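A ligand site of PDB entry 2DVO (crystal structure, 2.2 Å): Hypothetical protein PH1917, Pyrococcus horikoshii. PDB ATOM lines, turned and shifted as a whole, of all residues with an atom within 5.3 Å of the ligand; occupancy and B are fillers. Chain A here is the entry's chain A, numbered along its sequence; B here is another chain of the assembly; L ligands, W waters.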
ATOM      1  N   ILE A   6     -15.061 -13.575  13.398  1.00  0.00           N
ATOM      2  CA  ILE A   6     -14.365 -14.628  14.116  1.00  0.00           C
ATOM      3  C   ILE A   6     -15.389 -15.445  14.892  1.00  0.00           C
ATOM      4  O   ILE A   6     -15.905 -14.992  15.920  1.00  0.00           O
ATOM      5  CB  ILE A   6     -13.347 -14.059  15.123  1.00  0.00           C
ATOM      6  CG1 ILE A   6     -12.531 -12.942  14.459  1.00  0.00           C
ATOM      7  CG2 ILE A   6     -12.446 -15.166  15.651  1.00  0.00           C
ATOM      8  CD1 ILE A   6     -11.647 -13.400  13.348  1.00  0.00           C
ATOM      9  N   THR A   7     -15.698 -16.641  14.406  1.00  0.00           N
ATOM     10  CA  THR A   7     -16.653 -17.536  15.067  1.00  0.00           C
ATOM     11  C   THR A   7     -16.559 -18.957  14.528  1.00  0.00           C
ATOM     12  O   THR A   7     -16.125 -19.165  13.392  1.00  0.00           O
ATOM     13  CB  THR A   7     -18.115 -17.055  14.885  1.00  0.00           C
ATOM     14  OG1 THR A   7     -18.994 -17.942  15.584  1.00  0.00           O
ATOM     15  CG2 THR A   7     -18.496 -17.047  13.419  1.00  0.00           C
ATOM     16  N   SER A   8     -16.951 -19.924  15.343  1.00  0.00           N
ATOM     17  CA  SER A   8     -16.933 -21.312  14.920  1.00  0.00           C
ATOM     18  C   SER A   8     -18.373 -21.804  14.755  1.00  0.00           C
ATOM     19  O   SER A   8     -18.620 -22.991  14.553  1.00  0.00           O
ATOM     20  CB  SER A   8     -16.231 -22.189  15.967  1.00  0.00           C
ATOM     21  OG  SER A   8     -17.071 -22.372  17.103  1.00  0.00           O
ATOM     22  N   ASN A   9     -19.324 -20.871  14.821  1.00  0.00           N
ATOM     23  CA  ASN A   9     -20.748 -21.216  14.705  1.00  0.00           C
ATOM     24  C   ASN A   9     -21.306 -20.832  13.329  1.00  0.00           C
ATOM     25  O   ASN A   9     -21.629 -19.673  13.088  1.00  0.00           O
ATOM     26  CB  ASN A   9     -21.531 -20.502  15.802  1.00  0.00           C
ATOM     27  CG  ASN A   9     -22.940 -21.036  15.962  1.00  0.00           C
ATOM     28  OD1 ASN A   9     -23.706 -21.084  14.996  1.00  0.00           O
ATOM     29  ND2 ASN A   9     -23.301 -21.414  17.183  1.00  0.00           N
ATOM     30  N   LYS A  12     -24.554 -18.764  13.230  1.00  0.00           N
ATOM     31  CA  LYS A  12     -24.428 -17.311  13.420  1.00  0.00           C
ATOM     32  C   LYS A  12     -23.999 -16.650  12.114  1.00  0.00           C
ATOM     33  O   LYS A  12     -24.499 -15.584  11.746  1.00  0.00           O
ATOM     34  CB  LYS A  12     -23.370 -16.966  14.466  1.00  0.00           C
ATOM     35  CG  LYS A  12     -23.627 -17.395  15.887  1.00  0.00           C
ATOM     36  CD  LYS A  12     -22.478 -16.858  16.755  1.00  0.00           C
ATOM     37  CE  LYS A  12     -22.578 -17.253  18.219  1.00  0.00           C
ATOM     38  NZ  LYS A  12     -21.485 -16.587  18.991  1.00  0.00           N
ATOM     39  N   GLU A  15     -26.875 -16.265   9.599  1.00  0.00           N
ATOM     40  CA  GLU A  15     -27.774 -15.184  10.013  1.00  0.00           C
ATOM     41  C   GLU A  15     -27.140 -13.809   9.861  1.00  0.00           C
ATOM     42  O   GLU A  15     -27.767 -12.888   9.339  1.00  0.00           O
ATOM     43  CB  GLU A  15     -28.231 -15.421  11.452  1.00  0.00           C
ATOM     44  CG  GLU A  15     -29.320 -16.483  11.572  1.00  0.00           C
ATOM     45  CD  GLU A  15     -29.574 -16.919  12.986  1.00  0.00           C
ATOM     46  OE1 GLU A  15     -29.445 -16.096  13.906  1.00  0.00           O
ATOM     47  OE2 GLU A  15     -29.924 -18.096  13.181  1.00  0.00           O
ATOM     48  N   GLU A  33      -9.795 -19.485  17.036  1.00  0.00           N
ATOM     49  CA  GLU A  33     -10.199 -19.674  18.417  1.00  0.00           C
ATOM     50  C   GLU A  33      -9.570 -18.635  19.331  1.00  0.00           C
ATOM     51  O   GLU A  33      -8.391 -18.311  19.221  1.00  0.00           O
ATOM     52  CB  GLU A  33      -9.826 -21.077  18.887  1.00  0.00           C
ATOM     53  CG  GLU A  33     -10.791 -22.136  18.381  1.00  0.00           C
ATOM     54  CD  GLU A  33     -12.196 -21.914  18.913  1.00  0.00           C
ATOM     55  OE1 GLU A  33     -13.157 -22.440  18.303  1.00  0.00           O
ATOM     56  OE2 GLU A  33     -12.336 -21.215  19.942  1.00  0.00           O
ATOM     57  N   TYR A  34     -10.388 -18.093  20.234  1.00  0.00           N
ATOM     58  CA  TYR A  34      -9.927 -17.100  21.173  1.00  0.00           C
ATOM     59  C   TYR A  34     -10.501 -17.406  22.546  1.00  0.00           C
ATOM     60  O   TYR A  34     -11.524 -18.075  22.659  1.00  0.00           O
ATOM     61  CB  TYR A  34     -10.357 -15.700  20.712  1.00  0.00           C
ATOM     62  CG  TYR A  34     -11.854 -15.477  20.666  1.00  0.00           C
ATOM     63  CD1 TYR A  34     -12.539 -14.912  21.732  1.00  0.00           C
ATOM     64  CD2 TYR A  34     -12.590 -15.832  19.535  1.00  0.00           C
ATOM     65  CE1 TYR A  34     -13.929 -14.706  21.686  1.00  0.00           C
ATOM     66  CE2 TYR A  34     -13.964 -15.641  19.467  1.00  0.00           C
ATOM     67  CZ  TYR A  34     -14.639 -15.068  20.545  1.00  0.00           C
ATOM     68  OH  TYR A  34     -15.997 -14.884  20.475  1.00  0.00           O
ATOM     69  N   GLU A  36     -12.609 -17.390  25.626  1.00  0.00           N
ATOM     70  CA  GLU A  36     -13.941 -16.911  25.980  1.00  0.00           C
ATOM     71  C   GLU A  36     -14.041 -17.164  27.460  1.00  0.00           C
ATOM     72  O   GLU A  36     -14.304 -18.283  27.917  1.00  0.00           O
ATOM     73  CB  GLU A  36     -14.997 -17.680  25.195  1.00  0.00           C
ATOM     74  CG  GLU A  36     -14.952 -17.320  23.715  1.00  0.00           C
ATOM     75  CD  GLU A  36     -16.142 -17.846  22.953  1.00  0.00           C
ATOM     76  OE1 GLU A  36     -17.259 -17.843  23.514  1.00  0.00           O
ATOM     77  OE2 GLU A  36     -15.949 -18.241  21.780  1.00  0.00           O
ATOM     78  N   GLU A  64     -19.127 -12.475  18.346  1.00  0.00           N
ATOM     79  CA  GLU A  64     -20.436 -12.374  18.966  1.00  0.00           C
ATOM     80  C   GLU A  64     -20.567 -13.399  20.068  1.00  0.00           C
ATOM     81  O   GLU A  64     -20.066 -14.518  19.951  1.00  0.00           O
ATOM     82  CB  GLU A  64     -21.533 -12.575  17.935  1.00  0.00           C
ATOM     83  CG  GLU A  64     -22.912 -12.188  18.454  1.00  0.00           C
ATOM     84  CD  GLU A  64     -23.784 -13.378  18.796  1.00  0.00           C
ATOM     85  OE1 GLU A  64     -23.261 -14.354  19.393  1.00  0.00           O
ATOM     86  OE2 GLU A  64     -24.994 -13.337  18.471  1.00  0.00           O
ATOM     87  N   ASP A  65     -21.212 -13.008  21.152  1.00  0.00           N
ATOM     88  CA  ASP A  65     -21.459 -13.922  22.256  1.00  0.00           C
ATOM     89  C   ASP A  65     -22.949 -13.789  22.560  1.00  0.00           C
ATOM     90  O   ASP A  65     -23.492 -12.691  22.592  1.00  0.00           O
ATOM     91  CB  ASP A  65     -20.609 -13.542  23.481  1.00  0.00           C
ATOM     92  CG  ASP A  65     -20.281 -14.755  24.350  1.00  0.00           C
ATOM     93  OD1 ASP A  65     -19.745 -15.745  23.813  1.00  0.00           O
ATOM     94  OD2 ASP A  65     -20.554 -14.718  25.564  1.00  0.00           O
ATOM     95  N   SER A  66     -23.624 -14.920  22.770  1.00  0.00           N
ATOM     96  CA  SER A  66     -25.048 -14.872  23.026  1.00  0.00           C
ATOM     97  C   SER A  66     -25.443 -16.059  23.858  1.00  0.00           C
ATOM     98  O   SER A  66     -24.649 -16.980  24.073  1.00  0.00           O
ATOM     99  CB  SER A  66     -25.804 -14.862  21.703  1.00  0.00           C
ATOM    100  OG  SER A  66     -25.278 -15.823  20.803  1.00  0.00           O
ATOM    101  N   GLY A  67     -26.680 -16.052  24.335  1.00  0.00           N
ATOM    102  CA  GLY A  67     -27.177 -17.146  25.134  1.00  0.00           C
ATOM    103  C   GLY A  67     -28.656 -17.057  25.414  1.00  0.00           C
ATOM    104  O   GLY A  67     -29.304 -16.056  25.114  1.00  0.00           O
ATOM    105  N   LEU A  68     -29.198 -18.130  25.979  1.00  0.00           N
ATOM    106  CA  LEU A  68     -30.607 -18.194  26.356  1.00  0.00           C
ATOM    107  C   LEU A  68     -30.631 -18.070  27.880  1.00  0.00           C
ATOM    108  O   LEU A  68     -29.935 -18.824  28.571  1.00  0.00           O
ATOM    109  CB  LEU A  68     -31.207 -19.522  25.918  1.00  0.00           C
ATOM    110  CG  LEU A  68     -32.623 -19.863  26.399  1.00  0.00           C
ATOM    111  CD1 LEU A  68     -33.623 -18.835  25.853  1.00  0.00           C
ATOM    112  CD2 LEU A  68     -32.990 -21.270  25.929  1.00  0.00           C
ATOM    113  N   VAL A  79     -24.642 -17.404  29.612  1.00  0.00           N
ATOM    114  CA  VAL A  79     -23.323 -17.333  28.981  1.00  0.00           C
ATOM    115  C   VAL A  79     -22.797 -18.717  28.580  1.00  0.00           C
ATOM    116  O   VAL A  79     -22.011 -18.870  27.650  1.00  0.00           O
ATOM    117  CB  VAL A  79     -22.357 -16.672  29.961  1.00  0.00           C
ATOM    118  CG1 VAL A  79     -20.941 -16.712  29.395  1.00  0.00           C
ATOM    119  CG2 VAL A  79     -22.766 -15.229  30.199  1.00  0.00           C
ATOM    120  N   SER A  81     -24.580 -21.257  27.481  1.00  0.00           N
ATOM    121  CA  SER A  81     -25.596 -21.909  26.666  1.00  0.00           C
ATOM    122  C   SER A  81     -25.034 -23.007  25.758  1.00  0.00           C
ATOM    123  O   SER A  81     -25.652 -24.059  25.566  1.00  0.00           O
ATOM    124  CB  SER A  81     -26.347 -20.879  25.815  1.00  0.00           C
ATOM    125  OG  SER A  81     -27.131 -20.035  26.641  1.00  0.00           O
ATOM    126  N   SER A  82     -23.856 -22.762  25.189  1.00  0.00           N
ATOM    127  CA  SER A  82     -23.239 -23.732  24.291  1.00  0.00           C
ATOM    128  C   SER A  82     -22.922 -25.051  24.996  1.00  0.00           C
ATOM    129  O   SER A  82     -23.305 -26.126  24.518  1.00  0.00           O
ATOM    130  CB  SER A  82     -21.962 -23.158  23.690  1.00  0.00           C
ATOM    131  OG  SER A  82     -21.375 -24.080  22.789  1.00  0.00           O
ATOM    132  N   TYR A  85     -26.014 -26.916  26.004  1.00  0.00           N
ATOM    133  CA  TYR A  85     -26.697 -27.497  24.861  1.00  0.00           C
ATOM    134  C   TYR A  85     -26.060 -28.818  24.485  1.00  0.00           C
ATOM    135  O   TYR A  85     -26.740 -29.805  24.199  1.00  0.00           O
ATOM    136  CB  TYR A  85     -26.629 -26.567  23.653  1.00  0.00           C
ATOM    137  CG  TYR A  85     -27.202 -27.208  22.407  1.00  0.00           C
ATOM    138  CD1 TYR A  85     -28.578 -27.341  22.240  1.00  0.00           C
ATOM    139  CD2 TYR A  85     -26.365 -27.716  21.418  1.00  0.00           C
ATOM    140  CE1 TYR A  85     -29.116 -27.971  21.117  1.00  0.00           C
ATOM    141  CE2 TYR A  85     -26.880 -28.365  20.295  1.00  0.00           C
ATOM    142  CZ  TYR A  85     -28.256 -28.489  20.148  1.00  0.00           C
ATOM    143  OH  TYR A  85     -28.768 -29.120  19.036  1.00  0.00           O
ATOM    144  N   PHE A 107     -33.474 -14.373  24.784  1.00  0.00           N
ATOM    145  CA  PHE A 107     -32.234 -14.630  24.073  1.00  0.00           C
ATOM    146  C   PHE A 107     -31.575 -13.261  24.013  1.00  0.00           C
ATOM    147  O   PHE A 107     -32.259 -12.253  23.826  1.00  0.00           O
ATOM    148  CB  PHE A 107     -32.500 -15.102  22.642  1.00  0.00           C
ATOM    149  CG  PHE A 107     -32.416 -16.580  22.459  1.00  0.00           C
ATOM    150  CD1 PHE A 107     -31.233 -17.261  22.718  1.00  0.00           C
ATOM    151  CD2 PHE A 107     -33.513 -17.287  21.967  1.00  0.00           C
ATOM    152  CE1 PHE A 107     -31.132 -18.630  22.489  1.00  0.00           C
ATOM    153  CE2 PHE A 107     -33.418 -18.669  21.733  1.00  0.00           C
ATOM    154  CZ  PHE A 107     -32.234 -19.332  21.990  1.00  0.00           C
ATOM    155  N   PHE A 140     -30.729 -23.345  14.786  1.00  0.00           N
ATOM    156  CA  PHE A 140     -29.790 -24.212  15.499  1.00  0.00           C
ATOM    157  C   PHE A 140     -29.985 -24.055  16.994  1.00  0.00           C
ATOM    158  O   PHE A 140     -30.838 -23.287  17.437  1.00  0.00           O
ATOM    159  CB  PHE A 140     -28.361 -23.808  15.137  1.00  0.00           C
ATOM    160  CG  PHE A 140     -28.008 -22.403  15.544  1.00  0.00           C
ATOM    161  CD1 PHE A 140     -27.352 -22.163  16.746  1.00  0.00           C
ATOM    162  CD2 PHE A 140     -28.346 -21.319  14.745  1.00  0.00           C
ATOM    163  CE1 PHE A 140     -27.026 -20.877  17.131  1.00  0.00           C
ATOM    164  CE2 PHE A 140     -28.033 -20.016  15.122  1.00  0.00           C
ATOM    165  CZ  PHE A 140     -27.367 -19.796  16.318  1.00  0.00           C
ATOM    166  N   GLY A 141     -29.190 -24.784  17.761  1.00  0.00           N
ATOM    167  CA  GLY A 141     -29.260 -24.692  19.210  1.00  0.00           C
ATOM    168  C   GLY A 141     -30.640 -24.845  19.826  1.00  0.00           C
ATOM    169  O   GLY A 141     -31.363 -25.800  19.550  1.00  0.00           O
ATOM    170  N   TYR A 142     -31.002 -23.867  20.656  1.00  0.00           N
ATOM    171  CA  TYR A 142     -32.269 -23.851  21.382  1.00  0.00           C
ATOM    172  C   TYR A 142     -33.484 -23.390  20.573  1.00  0.00           C
ATOM    173  O   TYR A 142     -34.583 -23.268  21.122  1.00  0.00           O
ATOM    174  CB  TYR A 142     -32.140 -22.980  22.628  1.00  0.00           C
ATOM    175  CG  TYR A 142     -31.077 -23.439  23.611  1.00  0.00           C
ATOM    176  CD1 TYR A 142     -31.373 -24.381  24.590  1.00  0.00           C
ATOM    177  CD2 TYR A 142     -29.781 -22.939  23.545  1.00  0.00           C
ATOM    178  CE1 TYR A 142     -30.412 -24.807  25.483  1.00  0.00           C
ATOM    179  CE2 TYR A 142     -28.804 -23.372  24.438  1.00  0.00           C
ATOM    180  CZ  TYR A 142     -29.134 -24.302  25.405  1.00  0.00           C
ATOM    181  OH  TYR A 142     -28.162 -24.747  26.292  1.00  0.00           O
ATOM    182  N   ASP A 143     -33.302 -23.136  19.289  1.00  0.00           N
ATOM    183  CA  ASP A 143     -34.409 -22.683  18.458  1.00  0.00           C
ATOM    184  C   ASP A 143     -35.677 -23.549  18.542  1.00  0.00           C
ATOM    185  O   ASP A 143     -36.785 -23.019  18.558  1.00  0.00           O
ATOM    186  CB  ASP A 143     -33.969 -22.566  16.987  1.00  0.00           C
ATOM    187  CG  ASP A 143     -33.123 -21.321  16.728  1.00  0.00           C
ATOM    188  OD1 ASP A 143     -33.124 -20.399  17.567  1.00  0.00           O
ATOM    189  OD2 ASP A 143     -32.457 -21.254  15.670  1.00  0.00           O
ATOM    190  N   PHE A 155     -38.333 -20.518  17.098  1.00  0.00           N
ATOM    191  CA  PHE A 155     -37.363 -19.994  16.140  1.00  0.00           C
ATOM    192  C   PHE A 155     -37.054 -21.041  15.061  1.00  0.00           C
ATOM    193  O   PHE A 155     -36.814 -20.695  13.900  1.00  0.00           O
ATOM    194  CB  PHE A 155     -36.054 -19.605  16.838  1.00  0.00           C
ATOM    195  CG  PHE A 155     -36.040 -18.199  17.391  1.00  0.00           C
ATOM    196  CD1 PHE A 155     -36.950 -17.237  16.949  1.00  0.00           C
ATOM    197  CD2 PHE A 155     -35.071 -17.815  18.316  1.00  0.00           C
ATOM    198  CE1 PHE A 155     -36.885 -15.928  17.414  1.00  0.00           C
ATOM    199  CE2 PHE A 155     -35.001 -16.511  18.788  1.00  0.00           C
ATOM    200  CZ  PHE A 155     -35.906 -15.562  18.333  1.00  0.00           C
ATOM    201  N   LYS A 163     -36.513 -15.106  11.228  1.00  0.00           N
ATOM    202  CA  LYS A 163     -35.874 -15.124  12.540  1.00  0.00           C
ATOM    203  C   LYS A 163     -35.145 -13.806  12.787  1.00  0.00           C
ATOM    204  O   LYS A 163     -35.312 -13.189  13.846  1.00  0.00           O
ATOM    205  CB  LYS A 163     -34.896 -16.300  12.662  1.00  0.00           C
ATOM    206  CG  LYS A 163     -34.225 -16.387  14.030  1.00  0.00           C
ATOM    207  CD  LYS A 163     -33.242 -17.538  14.082  1.00  0.00           C
ATOM    208  CE  LYS A 163     -32.461 -17.549  15.401  1.00  0.00           C
ATOM    209  NZ  LYS A 163     -31.431 -18.622  15.407  1.00  0.00           N
ATOM    210  N   HIS A 168     -32.834 -11.781  18.801  1.00  0.00           N
ATOM    211  CA  HIS A 168     -31.903 -10.959  19.555  1.00  0.00           C
ATOM    212  C   HIS A 168     -30.756 -10.557  18.615  1.00  0.00           C
ATOM    213  O   HIS A 168     -30.314  -9.414  18.612  1.00  0.00           O
ATOM    214  CB  HIS A 168     -31.365 -11.775  20.727  1.00  0.00           C
ATOM    215  CG  HIS A 168     -30.902 -13.147  20.348  1.00  0.00           C
ATOM    216  ND1 HIS A 168     -31.707 -14.029  19.663  1.00  0.00           N
ATOM    217  CD2 HIS A 168     -29.718 -13.781  20.529  1.00  0.00           C
ATOM    218  CE1 HIS A 168     -31.040 -15.149  19.435  1.00  0.00           C
ATOM    219  NE2 HIS A 168     -29.830 -15.023  19.946  1.00  0.00           N
ATOM    220  N   ARG A 169     -30.288 -11.516  17.825  1.00  0.00           N
ATOM    221  CA  ARG A 169     -29.198 -11.276  16.880  1.00  0.00           C
ATOM    222  C   ARG A 169     -29.623 -10.223  15.838  1.00  0.00           C
ATOM    223  O   ARG A 169     -28.842  -9.334  15.487  1.00  0.00           O
ATOM    224  CB  ARG A 169     -28.809 -12.591  16.187  1.00  0.00           C
ATOM    225  CG  ARG A 169     -27.617 -12.521  15.222  1.00  0.00           C
ATOM    226  CD  ARG A 169     -27.029 -13.903  14.934  1.00  0.00           C
ATOM    227  NE  ARG A 169     -26.491 -14.508  16.156  1.00  0.00           N
ATOM    228  CZ  ARG A 169     -27.092 -15.453  16.863  1.00  0.00           C
ATOM    229  NH1 ARG A 169     -28.252 -15.962  16.469  1.00  0.00           N
ATOM    230  NH2 ARG A 169     -26.548 -15.865  18.007  1.00  0.00           N
ATOM    231  N   GLN B  38     -13.576 -20.420  29.460  1.00  0.00           N
ATOM    232  CA  GLN B  38     -14.399 -21.567  29.117  1.00  0.00           C
ATOM    233  C   GLN B  38     -13.548 -22.623  28.418  1.00  0.00           C
ATOM    234  O   GLN B  38     -12.727 -22.341  27.560  1.00  0.00           O
ATOM    235  CB  GLN B  38     -15.519 -21.076  28.181  1.00  0.00           C
ATOM    236  CG  GLN B  38     -16.472 -20.110  28.872  1.00  0.00           C
ATOM    237  CD  GLN B  38     -17.402 -19.493  27.853  1.00  0.00           C
ATOM    238  OE1 GLN B  38     -18.013 -20.158  27.035  1.00  0.00           O
ATOM    239  NE2 GLN B  38     -17.531 -18.163  27.962  1.00  0.00           N
HETATM  240  P1  LIG L   1     -18.452 -18.806  18.754  1.00  0.00           P
HETATM  241  O1  LIG L   1     -18.966 -17.587  18.223  1.00  0.00           O
HETATM  242  O2  LIG L   1     -18.097 -18.688  20.186  1.00  0.00           O
HETATM  243  O3  LIG L   1     -17.265 -19.232  18.032  1.00  0.00           O
HETATM  244  P2  LIG L   1     -20.440 -20.669  19.911  1.00  0.00           P
HETATM  245  O4  LIG L   1     -21.758 -20.741  19.343  1.00  0.00           O
HETATM  246  O5  LIG L   1     -19.813 -21.875  20.445  1.00  0.00           O
HETATM  247  O6  LIG L   1     -19.496 -20.064  18.902  1.00  0.00           O
HETATM  248  P3  LIG L   1     -21.480 -18.917  21.878  1.00  0.00           P
HETATM  249  O7  LIG L   1     -20.578 -18.779  23.136  1.00  0.00           O
HETATM  250  O8  LIG L   1     -21.840 -17.489  21.431  1.00  0.00           O
HETATM  251  O9  LIG L   1     -20.378 -19.775  21.135  1.00  0.00           O
HETATM  252  O10 LIG L   1     -22.681 -19.906  22.221  1.00  0.00           O
HETATM  253  C1  LIG L   1     -23.971 -19.613  22.920  1.00  0.00           C
HETATM  254  C2  LIG L   1     -24.855 -20.588  22.614  1.00  0.00           C
HETATM  255  O11 LIG L   1     -26.040 -19.660  22.695  1.00  0.00           O
HETATM  256  C3  LIG L   1     -24.715 -21.367  21.278  1.00  0.00           C
HETATM  257  O12 LIG L   1     -23.874 -22.431  21.167  1.00  0.00           O
HETATM  258  C4  LIG L   1     -26.264 -21.514  21.009  1.00  0.00           C
HETATM  259  O13 LIG L   1     -26.535 -22.868  21.571  1.00  0.00           O
HETATM  260  C5  LIG L   1     -26.966 -20.379  21.732  1.00  0.00           C
HETATM  261  N1  LIG L   1     -27.594 -19.525  20.828  1.00  0.00           N
HETATM  262  C6  LIG L   1     -27.275 -18.226  20.418  1.00  0.00           C
HETATM  263  N2  LIG L   1     -28.022 -17.613  19.552  1.00  0.00           N
HETATM  264  C7  LIG L   1     -28.961 -18.609  19.366  1.00  0.00           C
HETATM  265  C8  LIG L   1     -30.084 -18.626  18.551  1.00  0.00           C
HETATM  266  O14 LIG L   1     -30.504 -17.670  17.731  1.00  0.00           O
HETATM  267  N3  LIG L   1     -30.919 -19.842  18.530  1.00  0.00           N
HETATM  268  C9  LIG L   1     -30.556 -20.934  19.363  1.00  0.00           C
HETATM  269  N4  LIG L   1     -29.497 -20.982  20.189  1.00  0.00           N
HETATM  270  C10 LIG L   1     -28.724 -19.792  20.136  1.00  0.00           C
HETATM  271  O   HOH W   1     -17.659 -15.040  17.907  1.00  0.00           O
HETATM  272  O   HOH W   2     -24.638 -24.893  20.912  1.00  0.00           O
HETATM  273  O   HOH W   3     -16.646 -21.013  21.947  1.00  0.00           O
HETATM  274  O   HOH W   4     -19.989 -17.545  26.289  1.00  0.00           O
HETATM  275  O   HOH W   5     -14.729 -18.704  18.097  1.00  0.00           O
HETATM  276  O   HOH W   6     -22.039 -20.546  25.440  1.00  0.00           O
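The side-chain carboxylate (OD1) of Asp 143 lies within hydrogen-bond range of a nitrogen (N3) of the ligand (2.5 Å).
NZ of Lys 12 is in salt-bridge range of O8 of the ligand.
OG1 of Thr 7 sits at hydrogen-bond distance from O1 of the ligand, at 2.7 Å.
The side-chain amino group of Lys 163 is in hydrogen-bond range of an oxygen (O14) of the ligand, 2.7 Å away.
An oxygen (O2) of the ligand sits close to the side-chain carboxylate (OE2) of Glu 36 (2.7 Å).
An oxygen (O4) of the ligand is in hydrogen-bond range of the side-chain amide nitrogen (ND2) of Asn 9 (2.7 Å).
The guanidinium group (NH2) of Arg 169 lies within hydrogen-bond range of a nitrogen (N2) of the ligand, at 2.8 Å.
The backbone NH of Ser 8 sits at hydrogen-bond distance from an oxygen (O3) of the ligand (2.8 Å).
An oxygen (O3) of the ligand is in hydrogen-bond range of the side-chain hydroxyl (OG) of Ser 8, 3.3 Å away.
The backbone NH (N) of Ser 66 is in hydrogen-bond range of an oxygen (O8) of the ligand (3.4 Å).
N2 of the ligand sits at hydrogen-bond distance from NE2 of His 168, at 3.2 Å.
N4 of the ligand lies close to N of Tyr 142 (3.3 Å).
OG of Ser 82 sits close to O12 of the ligand.
An oxygen (O7) of the ligand lies close to the side-chain carboxylate (OD1) of Asp 65.
Glu 64 touches the ligand.
Gly 67 touches the ligand.
CB of Ser 81 touches O11 of the ligand, at 3.4 Å.
Phe 107 touches the ligand (CZ to C9, 3.5 Å).
O of Phe 140 touches C9 of the ligand (3.1 Å).
CA of Gly 141 touches N4 of the ligand (3.8 Å).
Along chain A the residues within 4 Å of the ligand span positions 7 to 169.
The side-chain carboxylate of Asp 143 is in hydrogen-bond range of the backbone NH of Phe 140 (2.9 Å).
O of Asp 143 is in hydrogen-bond range of N of Phe 155, 3.3 Å away.
N of Asn 9 sits at hydrogen-bond distance from OG1 of Thr 7.
OE2 of Glu 15 lies within salt-bridge range of NZ of Lys 163, at 2.7 Å.
The guanidinium group (NH2) of Arg 169 is in hydrogen-bond range of the side-chain hydroxyl (OG) of Ser 66, at 3.1 Å.
NE of Arg 169 is in salt-bridge range of OE2 of Glu 64 (3.0 Å).
OE1 of Glu 15 lies within salt-bridge range of NH1 of Arg 169 (2.8 Å).
The side-chain hydroxyl of Ser 66 lies within hydrogen-bond range of the side-chain carboxylate of Glu 64, at 2.9 Å.
Water W1 lies within hydrogen-bond range of O of Ile 6 (2.7 Å), O1 of the ligand (2.9 Å), N of Glu 64 (3.0 Å) and OH of Tyr 34 (3.1 Å).
Water W6 lies within hydrogen-bond range of the backbone carbonyl oxygen of Val 79 (2.8 Å), the backbone NH of Ser 82 (2.9 Å), an oxygen (O7) of the ligand (3.3 Å) and the backbone NH of Ser 81 (3.3 Å).
Water W3 bridges the side-chain carboxylate of Glu 36 and an oxygen (O2) of the ligand.
Water W4 lies within hydrogen-bond range of the backbone carbonyl oxygen of Val 79 (2.8 Å), the side-chain carboxylate of Asp 65 (3.0 Å), the side-chain amide nitrogen of Gln 38 of chain B (3.0 Å) and an oxygen (O7) of the ligand (3.4 Å).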
